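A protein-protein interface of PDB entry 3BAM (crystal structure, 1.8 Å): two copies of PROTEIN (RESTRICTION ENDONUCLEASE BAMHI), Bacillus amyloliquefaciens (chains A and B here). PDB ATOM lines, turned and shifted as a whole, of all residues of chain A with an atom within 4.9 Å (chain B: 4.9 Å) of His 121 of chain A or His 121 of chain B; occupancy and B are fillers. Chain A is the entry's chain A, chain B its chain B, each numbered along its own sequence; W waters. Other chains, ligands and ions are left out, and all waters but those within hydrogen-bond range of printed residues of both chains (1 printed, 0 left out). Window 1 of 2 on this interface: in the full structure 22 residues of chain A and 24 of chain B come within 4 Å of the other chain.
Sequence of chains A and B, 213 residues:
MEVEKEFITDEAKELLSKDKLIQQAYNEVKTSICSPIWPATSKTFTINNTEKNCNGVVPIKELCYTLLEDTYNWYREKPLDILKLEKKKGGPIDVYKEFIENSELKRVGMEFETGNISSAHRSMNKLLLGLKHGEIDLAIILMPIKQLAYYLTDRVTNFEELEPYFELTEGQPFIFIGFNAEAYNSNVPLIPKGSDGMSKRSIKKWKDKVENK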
ATOM      1  N   ILE A 117     -24.804 -19.804  11.789  1.00  0.00           N
ATOM      2  CA  ILE A 117     -23.478 -19.184  11.717  1.00  0.00           C
ATOM      3  C   ILE A 117     -23.410 -17.844  12.488  1.00  0.00           C
ATOM      4  O   ILE A 117     -22.394 -17.543  13.122  1.00  0.00           O
ATOM      5  CB  ILE A 117     -22.994 -19.019  10.231  1.00  0.00           C
ATOM      6  CG1 ILE A 117     -21.670 -18.253  10.165  1.00  0.00           C
ATOM      7  CG2 ILE A 117     -24.037 -18.317   9.392  1.00  0.00           C
ATOM      8  CD1 ILE A 117     -20.480 -18.964  10.829  1.00  0.00           C
ATOM      9  N   SER A 118     -24.493 -17.065  12.481  1.00  0.00           N
ATOM     10  CA  SER A 118     -24.517 -15.791  13.207  1.00  0.00           C
ATOM     11  C   SER A 118     -24.339 -16.027  14.712  1.00  0.00           C
ATOM     12  O   SER A 118     -23.647 -15.273  15.401  1.00  0.00           O
ATOM     13  CB  SER A 118     -25.820 -15.030  12.927  1.00  0.00           C
ATOM     14  OG  SER A 118     -26.959 -15.828  13.185  1.00  0.00           O
ATOM     15  N   SER A 119     -24.915 -17.119  15.201  1.00  0.00           N
ATOM     16  CA  SER A 119     -24.817 -17.470  16.607  1.00  0.00           C
ATOM     17  C   SER A 119     -23.360 -17.755  16.990  1.00  0.00           C
ATOM     18  O   SER A 119     -22.963 -17.550  18.136  1.00  0.00           O
ATOM     19  CB  SER A 119     -25.714 -18.664  16.903  1.00  0.00           C
ATOM     20  OG  SER A 119     -26.046 -18.703  18.273  1.00  0.00           O
ATOM     21  N   ALA A 120     -22.565 -18.217  16.031  1.00  0.00           N
ATOM     22  CA  ALA A 120     -21.153 -18.485  16.264  1.00  0.00           C
ATOM     23  C   ALA A 120     -20.452 -17.179  16.622  1.00  0.00           C
ATOM     24  O   ALA A 120     -19.487 -17.175  17.381  1.00  0.00           O
ATOM     25  CB  ALA A 120     -20.514 -19.094  15.022  1.00  0.00           C
ATOM     26  N   HIS A 121     -20.939 -16.066  16.077  1.00  0.00           N
ATOM     27  CA  HIS A 121     -20.360 -14.761  16.368  1.00  0.00           C
ATOM     28  C   HIS A 121     -20.636 -14.392  17.818  1.00  0.00           C
ATOM     29  O   HIS A 121     -19.769 -13.851  18.505  1.00  0.00           O
ATOM     30  CB  HIS A 121     -20.915 -13.703  15.422  1.00  0.00           C
ATOM     31  CG  HIS A 121     -20.363 -13.793  14.042  1.00  0.00           C
ATOM     32  ND1 HIS A 121     -19.236 -13.099  13.642  1.00  0.00           N
ATOM     33  CD2 HIS A 121     -20.757 -14.514  12.963  1.00  0.00           C
ATOM     34  CE1 HIS A 121     -18.970 -13.389  12.387  1.00  0.00           C
ATOM     35  NE2 HIS A 121     -19.874 -14.247  11.949  1.00  0.00           N
ATOM     36  N   ARG A 122     -21.841 -14.689  18.292  1.00  0.00           N
ATOM     37  CA  ARG A 122     -22.180 -14.410  19.682  1.00  0.00           C
ATOM     38  C   ARG A 122     -21.280 -15.267  20.585  1.00  0.00           C
ATOM     39  O   ARG A 122     -20.674 -14.749  21.520  1.00  0.00           O
ATOM     40  CB  ARG A 122     -23.669 -14.684  19.941  1.00  0.00           C
ATOM     41  CG  ARG A 122     -24.103 -14.549  21.406  1.00  0.00           C
ATOM     42  CD  ARG A 122     -25.606 -14.718  21.568  1.00  0.00           C
ATOM     43  NE  ARG A 122     -26.112 -15.946  20.957  1.00  0.00           N
ATOM     44  CZ  ARG A 122     -27.387 -16.148  20.631  1.00  0.00           C
ATOM     45  NH1 ARG A 122     -28.290 -15.199  20.851  1.00  0.00           N
ATOM     46  NH2 ARG A 122     -27.765 -17.284  20.057  1.00  0.00           N
ATOM     47  N   SER A 123     -21.141 -16.553  20.269  1.00  0.00           N
ATOM     48  CA  SER A 123     -20.291 -17.444  21.053  1.00  0.00           C
ATOM     49  C   SER A 123     -18.849 -16.946  21.106  1.00  0.00           C
ATOM     50  O   SER A 123     -18.260 -16.849  22.188  1.00  0.00           O
ATOM     51  CB  SER A 123     -20.343 -18.868  20.498  1.00  0.00           C
ATOM     52  OG  SER A 123     -21.653 -19.405  20.613  1.00  0.00           O
ATOM     53  N   MET A 124     -18.278 -16.609  19.953  1.00  0.00           N
ATOM     54  CA  MET A 124     -16.908 -16.114  19.904  1.00  0.00           C
ATOM     55  C   MET A 124     -16.738 -14.831  20.722  1.00  0.00           C
ATOM     56  O   MET A 124     -15.722 -14.656  21.398  1.00  0.00           O
ATOM     57  CB  MET A 124     -16.472 -15.880  18.462  1.00  0.00           C
ATOM     58  CG  MET A 124     -15.051 -15.343  18.335  1.00  0.00           C
ATOM     59  SD  MET A 124     -14.517 -15.124  16.647  1.00  0.00           S
ATOM     60  CE  MET A 124     -15.361 -13.574  16.215  1.00  0.00           C
ATOM     61  N   ASN A 125     -17.724 -13.935  20.667  1.00  0.00           N
ATOM     62  CA  ASN A 125     -17.667 -12.681  21.421  1.00  0.00           C
ATOM     63  C   ASN A 125     -17.777 -12.883  22.931  1.00  0.00           C
ATOM     64  O   ASN A 125     -17.156 -12.151  23.706  1.00  0.00           O
ATOM     65  CB  ASN A 125     -18.749 -11.716  20.938  1.00  0.00           C
ATOM     66  CG  ASN A 125     -18.483 -11.191  19.534  1.00  0.00           C
ATOM     67  OD1 ASN A 125     -19.403 -10.737  18.856  1.00  0.00           O
ATOM     68  ND2 ASN A 125     -17.224 -11.221  19.108  1.00  0.00           N
ATOM     69  N   LEU A 162     -16.818 -18.883   9.463  1.00  0.00           N
ATOM     70  CA  LEU A 162     -16.417 -18.065  10.606  1.00  0.00           C
ATOM     71  C   LEU A 162     -14.941 -17.723  10.467  1.00  0.00           C
ATOM     72  O   LEU A 162     -14.476 -16.723  10.993  1.00  0.00           O
ATOM     73  CB  LEU A 162     -16.668 -18.801  11.926  1.00  0.00           C
ATOM     74  CG  LEU A 162     -16.358 -18.051  13.224  1.00  0.00           C
ATOM     75  CD1 LEU A 162     -17.219 -16.808  13.333  1.00  0.00           C
ATOM     76  CD2 LEU A 162     -16.583 -18.970  14.411  1.00  0.00           C
ATOM     77  N   TYR A 165     -13.221 -14.333  10.287  1.00  0.00           N
ATOM     78  CA  TYR A 165     -13.299 -13.543  11.509  1.00  0.00           C
ATOM     79  C   TYR A 165     -12.391 -14.050  12.625  1.00  0.00           C
ATOM     80  O   TYR A 165     -12.316 -13.426  13.678  1.00  0.00           O
ATOM     81  CB  TYR A 165     -14.746 -13.480  12.019  1.00  0.00           C
ATOM     82  CG  TYR A 165     -15.696 -12.770  11.078  1.00  0.00           C
ATOM     83  CD1 TYR A 165     -15.935 -11.406  11.197  1.00  0.00           C
ATOM     84  CD2 TYR A 165     -16.319 -13.456  10.041  1.00  0.00           C
ATOM     85  CE1 TYR A 165     -16.770 -10.743  10.298  1.00  0.00           C
ATOM     86  CE2 TYR A 165     -17.153 -12.800   9.136  1.00  0.00           C
ATOM     87  CZ  TYR A 165     -17.370 -11.446   9.273  1.00  0.00           C
ATOM     88  OH  TYR A 165     -18.184 -10.793   8.387  1.00  0.00           O
ATOM     89  N   ILE B 117     -30.794 -11.439  17.155  1.00  0.00           N
ATOM     90  CA  ILE B 117     -29.734 -10.851  17.971  1.00  0.00           C
ATOM     91  C   ILE B 117     -28.338 -11.414  17.654  1.00  0.00           C
ATOM     92  O   ILE B 117     -27.347 -10.690  17.714  1.00  0.00           O
ATOM     93  CB  ILE B 117     -30.070 -10.959  19.504  1.00  0.00           C
ATOM     94  CG1 ILE B 117     -28.974 -10.315  20.350  1.00  0.00           C
ATOM     95  CG2 ILE B 117     -30.311 -12.400  19.923  1.00  0.00           C
ATOM     96  CD1 ILE B 117     -28.806  -8.834  20.120  1.00  0.00           C
ATOM     97  N   SER B 118     -28.255 -12.688  17.288  1.00  0.00           N
ATOM     98  CA  SER B 118     -26.969 -13.297  16.948  1.00  0.00           C
ATOM     99  C   SER B 118     -26.392 -12.652  15.692  1.00  0.00           C
ATOM    100  O   SER B 118     -25.179 -12.457  15.586  1.00  0.00           O
ATOM    101  CB  SER B 118     -27.108 -14.809  16.761  1.00  0.00           C
ATOM    102  OG  SER B 118     -28.088 -15.150  15.794  1.00  0.00           O
ATOM    103  N   SER B 119     -27.272 -12.282  14.762  1.00  0.00           N
ATOM    104  CA  SER B 119     -26.857 -11.644  13.520  1.00  0.00           C
ATOM    105  C   SER B 119     -26.239 -10.284  13.842  1.00  0.00           C
ATOM    106  O   SER B 119     -25.299  -9.865  13.169  1.00  0.00           O
ATOM    107  CB  SER B 119     -28.037 -11.497  12.550  1.00  0.00           C
ATOM    108  OG  SER B 119     -27.635 -10.937  11.309  1.00  0.00           O
ATOM    109  N   ALA B 120     -26.737  -9.609  14.883  1.00  0.00           N
ATOM    110  CA  ALA B 120     -26.191  -8.308  15.298  1.00  0.00           C
ATOM    111  C   ALA B 120     -24.716  -8.470  15.646  1.00  0.00           C
ATOM    112  O   ALA B 120     -23.922  -7.548  15.455  1.00  0.00           O
ATOM    113  CB  ALA B 120     -26.954  -7.756  16.484  1.00  0.00           C
ATOM    114  N   HIS B 121     -24.347  -9.651  16.141  1.00  0.00           N
ATOM    115  CA  HIS B 121     -22.954  -9.959  16.478  1.00  0.00           C
ATOM    116  C   HIS B 121     -22.101 -10.045  15.195  1.00  0.00           C
ATOM    117  O   HIS B 121     -20.969  -9.538  15.147  1.00  0.00           O
ATOM    118  CB  HIS B 121     -22.871 -11.263  17.288  1.00  0.00           C
ATOM    119  CG  HIS B 121     -23.327 -11.119  18.708  1.00  0.00           C
ATOM    120  ND1 HIS B 121     -22.457 -10.849  19.747  1.00  0.00           N
ATOM    121  CD2 HIS B 121     -24.559 -11.181  19.265  1.00  0.00           C
ATOM    122  CE1 HIS B 121     -23.132 -10.751  20.871  1.00  0.00           C
ATOM    123  NE2 HIS B 121     -24.419 -10.947  20.608  1.00  0.00           N
ATOM    124  N   ARG B 122     -22.647 -10.667  14.153  1.00  0.00           N
ATOM    125  CA  ARG B 122     -21.941 -10.770  12.882  1.00  0.00           C
ATOM    126  C   ARG B 122     -21.790  -9.356  12.317  1.00  0.00           C
ATOM    127  O   ARG B 122     -20.688  -8.967  11.932  1.00  0.00           O
ATOM    128  CB  ARG B 122     -22.689 -11.679  11.899  1.00  0.00           C
ATOM    129  CG  ARG B 122     -22.102 -11.694  10.485  1.00  0.00           C
ATOM    130  CD  ARG B 122     -22.808 -12.708   9.612  1.00  0.00           C
ATOM    131  NE  ARG B 122     -24.252 -12.489   9.566  1.00  0.00           N
ATOM    132  CZ  ARG B 122     -25.143 -13.441   9.307  1.00  0.00           C
ATOM    133  NH1 ARG B 122     -24.736 -14.678   9.070  1.00  0.00           N
ATOM    134  NH2 ARG B 122     -26.444 -13.182   9.369  1.00  0.00           N
ATOM    135  N   SER B 123     -22.880  -8.585  12.301  1.00  0.00           N
ATOM    136  CA  SER B 123     -22.854  -7.202  11.810  1.00  0.00           C
ATOM    137  C   SER B 123     -21.787  -6.356  12.513  1.00  0.00           C
ATOM    138  O   SER B 123     -21.015  -5.642  11.870  1.00  0.00           O
ATOM    139  CB  SER B 123     -24.230  -6.555  11.976  1.00  0.00           C
ATOM    140  OG  SER B 123     -25.192  -7.230  11.186  1.00  0.00           O
ATOM    141  N   MET B 124     -21.724  -6.465  13.834  1.00  0.00           N
ATOM    142  CA  MET B 124     -20.745  -5.733  14.606  1.00  0.00           C
ATOM    143  C   MET B 124     -19.335  -6.206  14.258  1.00  0.00           C
ATOM    144  O   MET B 124     -18.427  -5.394  14.084  1.00  0.00           O
ATOM    145  CB  MET B 124     -21.014  -5.914  16.096  1.00  0.00           C
ATOM    146  CG  MET B 124     -20.209  -4.973  16.959  1.00  0.00           C
ATOM    147  SD  MET B 124     -20.460  -5.248  18.683  1.00  0.00           S
ATOM    148  CE  MET B 124     -19.172  -6.442  19.001  1.00  0.00           C
ATOM    149  N   ASN B 125     -19.147  -7.516  14.144  1.00  0.00           N
ATOM    150  CA  ASN B 125     -17.837  -8.064  13.806  1.00  0.00           C
ATOM    151  C   ASN B 125     -17.346  -7.654  12.415  1.00  0.00           C
ATOM    152  O   ASN B 125     -16.159  -7.396  12.222  1.00  0.00           O
ATOM    153  CB  ASN B 125     -17.847  -9.589  13.920  1.00  0.00           C
ATOM    154  CG  ASN B 125     -17.873 -10.071  15.354  1.00  0.00           C
ATOM    155  OD1 ASN B 125     -18.186 -11.236  15.605  1.00  0.00           O
ATOM    156  ND2 ASN B 125     -17.522  -9.201  16.297  1.00  0.00           N
ATOM    157  N   LEU B 162     -27.575  -6.591  23.017  1.00  0.00           N
ATOM    158  CA  LEU B 162     -26.244  -6.478  22.415  1.00  0.00           C
ATOM    159  C   LEU B 162     -25.332  -5.590  23.274  1.00  0.00           C
ATOM    160  O   LEU B 162     -24.101  -5.700  23.224  1.00  0.00           O
ATOM    161  CB  LEU B 162     -26.345  -5.920  20.992  1.00  0.00           C
ATOM    162  CG  LEU B 162     -25.058  -5.776  20.168  1.00  0.00           C
ATOM    163  CD1 LEU B 162     -24.393  -7.126  19.942  1.00  0.00           C
ATOM    164  CD2 LEU B 162     -25.380  -5.111  18.835  1.00  0.00           C
ATOM    165  N   TYR B 165     -21.947  -6.314  24.927  1.00  0.00           N
ATOM    166  CA  TYR B 165     -20.855  -6.508  23.983  1.00  0.00           C
ATOM    167  C   TYR B 165     -20.285  -5.246  23.338  1.00  0.00           C
ATOM    168  O   TYR B 165     -19.246  -5.296  22.680  1.00  0.00           O
ATOM    169  CB  TYR B 165     -21.293  -7.502  22.915  1.00  0.00           C
ATOM    170  CG  TYR B 165     -21.667  -8.849  23.487  1.00  0.00           C
ATOM    171  CD1 TYR B 165     -20.705  -9.835  23.671  1.00  0.00           C
ATOM    172  CD2 TYR B 165     -22.982  -9.141  23.843  1.00  0.00           C
ATOM    173  CE1 TYR B 165     -21.034 -11.086  24.187  1.00  0.00           C
ATOM    174  CE2 TYR B 165     -23.322 -10.382  24.364  1.00  0.00           C
ATOM    175  CZ  TYR B 165     -22.347 -11.364  24.533  1.00  0.00           C
ATOM    176  OH  TYR B 165     -22.699 -12.613  24.997  1.00  0.00           O
HETATM  177  O   HOH W   1     -15.471  -9.334  18.200  1.00  0.00           O
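OG of Ser 119 of chain A is in hydrogen-bond range of NH2 of Arg 122 of chain A, 2.9 Å away. The backbone carbonyl oxygen (O) of His 121 of chain B sits close to the side-chain amide oxygen (OD1) of Asn 125 of chain B, 3.3 Å away. The backbone carbonyl oxygen of Ser 119 of chain B sits at hydrogen-bond distance from the side-chain hydroxyl of Ser 123 of chain B (3.3 Å). The backbone carbonyl oxygen of Ser 119 of chain A is in hydrogen-bond range of the side-chain hydroxyl of Ser 123 of chain A. The backbone carbonyl oxygen of His 121 of chain A lies close to the side-chain amide oxygen of Asn 125 of chain A, at 3.2 Å. The side-chain hydroxyl (OG) of Ser 119 of chain B lies within hydrogen-bond range of the guanidinium group (NH2) of Arg 122 of chain B, 3.2 Å away.
Of chain B, only His 121, Arg 122 and Asn 125 come within 4 Å of His 121 of chain A. Of the printed residues of chain A, Ser 119 of chain B touches Ser 118. Of the printed residues of chain A, Asn 125 of chain B touches His 121, Met 124, Asn 125 and Tyr 165.
OD1 of Asn 125 of chain A is in hydrogen-bond range of ND1 of His 121 of chain B (3.2 Å). ND2 of Asn 125 of chain A lies close to ND2 of Asn 125 of chain B, 3.5 Å away. The side-chain hydroxyl of Ser 118 of chain A lies within hydrogen-bond range of the side-chain hydroxyl of Ser 118 of chain B, at 2.9 Å. The side-chain amide oxygen of Asn 125 of chain B sits at hydrogen-bond distance from a ring nitrogen (ND1) of His 121 of chain A, at 2.9 Å.
Of the 11 printed residues of chain B, 7 touch a printed residue of chain A. Hydrophobic or aromatic side chains of chain B within 4 Å of the printed part of chain A: Ile 117, His 121 and Tyr 165. Of the 11 printed residues of chain A, 8 touch a printed residue of chain B. Hydrophobic or aromatic side chains of chain A within 4 Å of the printed part of chain B: Ile 117, His 121, Met 124 and Tyr 165. Among the printed residues, 14 pairs touch across the chains. Among the printed residues, no Asp or Glu carboxylate lies within 4 Å of a Lys or Arg side-chain nitrogen of the other chain.
Water W1 lies within hydrogen-bond range of ND2 of Asn 125 of chain A (2.7 Å) and ND2 of Asn 125 of chain B (2.8 Å).
Ser 118 of chain A touches Ser 119 of chain B, and with the chains exchanged Ser 119 of chain A touches Ser 118 of chain B. His 121 of chain A touches its own counterpart, His 121 of chain B. His 121 of chain A touches Arg 122 of chain B, and with the chains exchanged Arg 122 of chain A touches His 121 of chain B. Met 124 of chain A touches Asn 125 of chain B, but with the chains exchanged Asn 125 of chain A does not touch Met 124 of chain B (4.3 Å). Positions printed for both chains: 117, 118, 119, 120, 121, 122, 123, 124, 125, 162 and 165. Of the 14 pairs that touch across the chains among the printed residues, 13 have their exchanged pair printed and touching as well.
Among the printed residues, merely in contact across the chains: Ile 117 of chain A with Arg 122 of chain B, Ser 118 of chain A with Ser 119 of chain B, Ser 119 of chain A with Ser 118 of chain B, His 121 of chain A with His 121 of chain B, His 121 of chain A with Arg 122 of chain B, Arg 122 of chain A with Ile 117 of chain B, Arg 122 of chain A with His 121 of chain B, Met 124 of chain A with Asn 125 of chain B, Asn 125 of chain A with Tyr 165 of chain B and Tyr 165 of chain A with Asn 125 of chain B.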
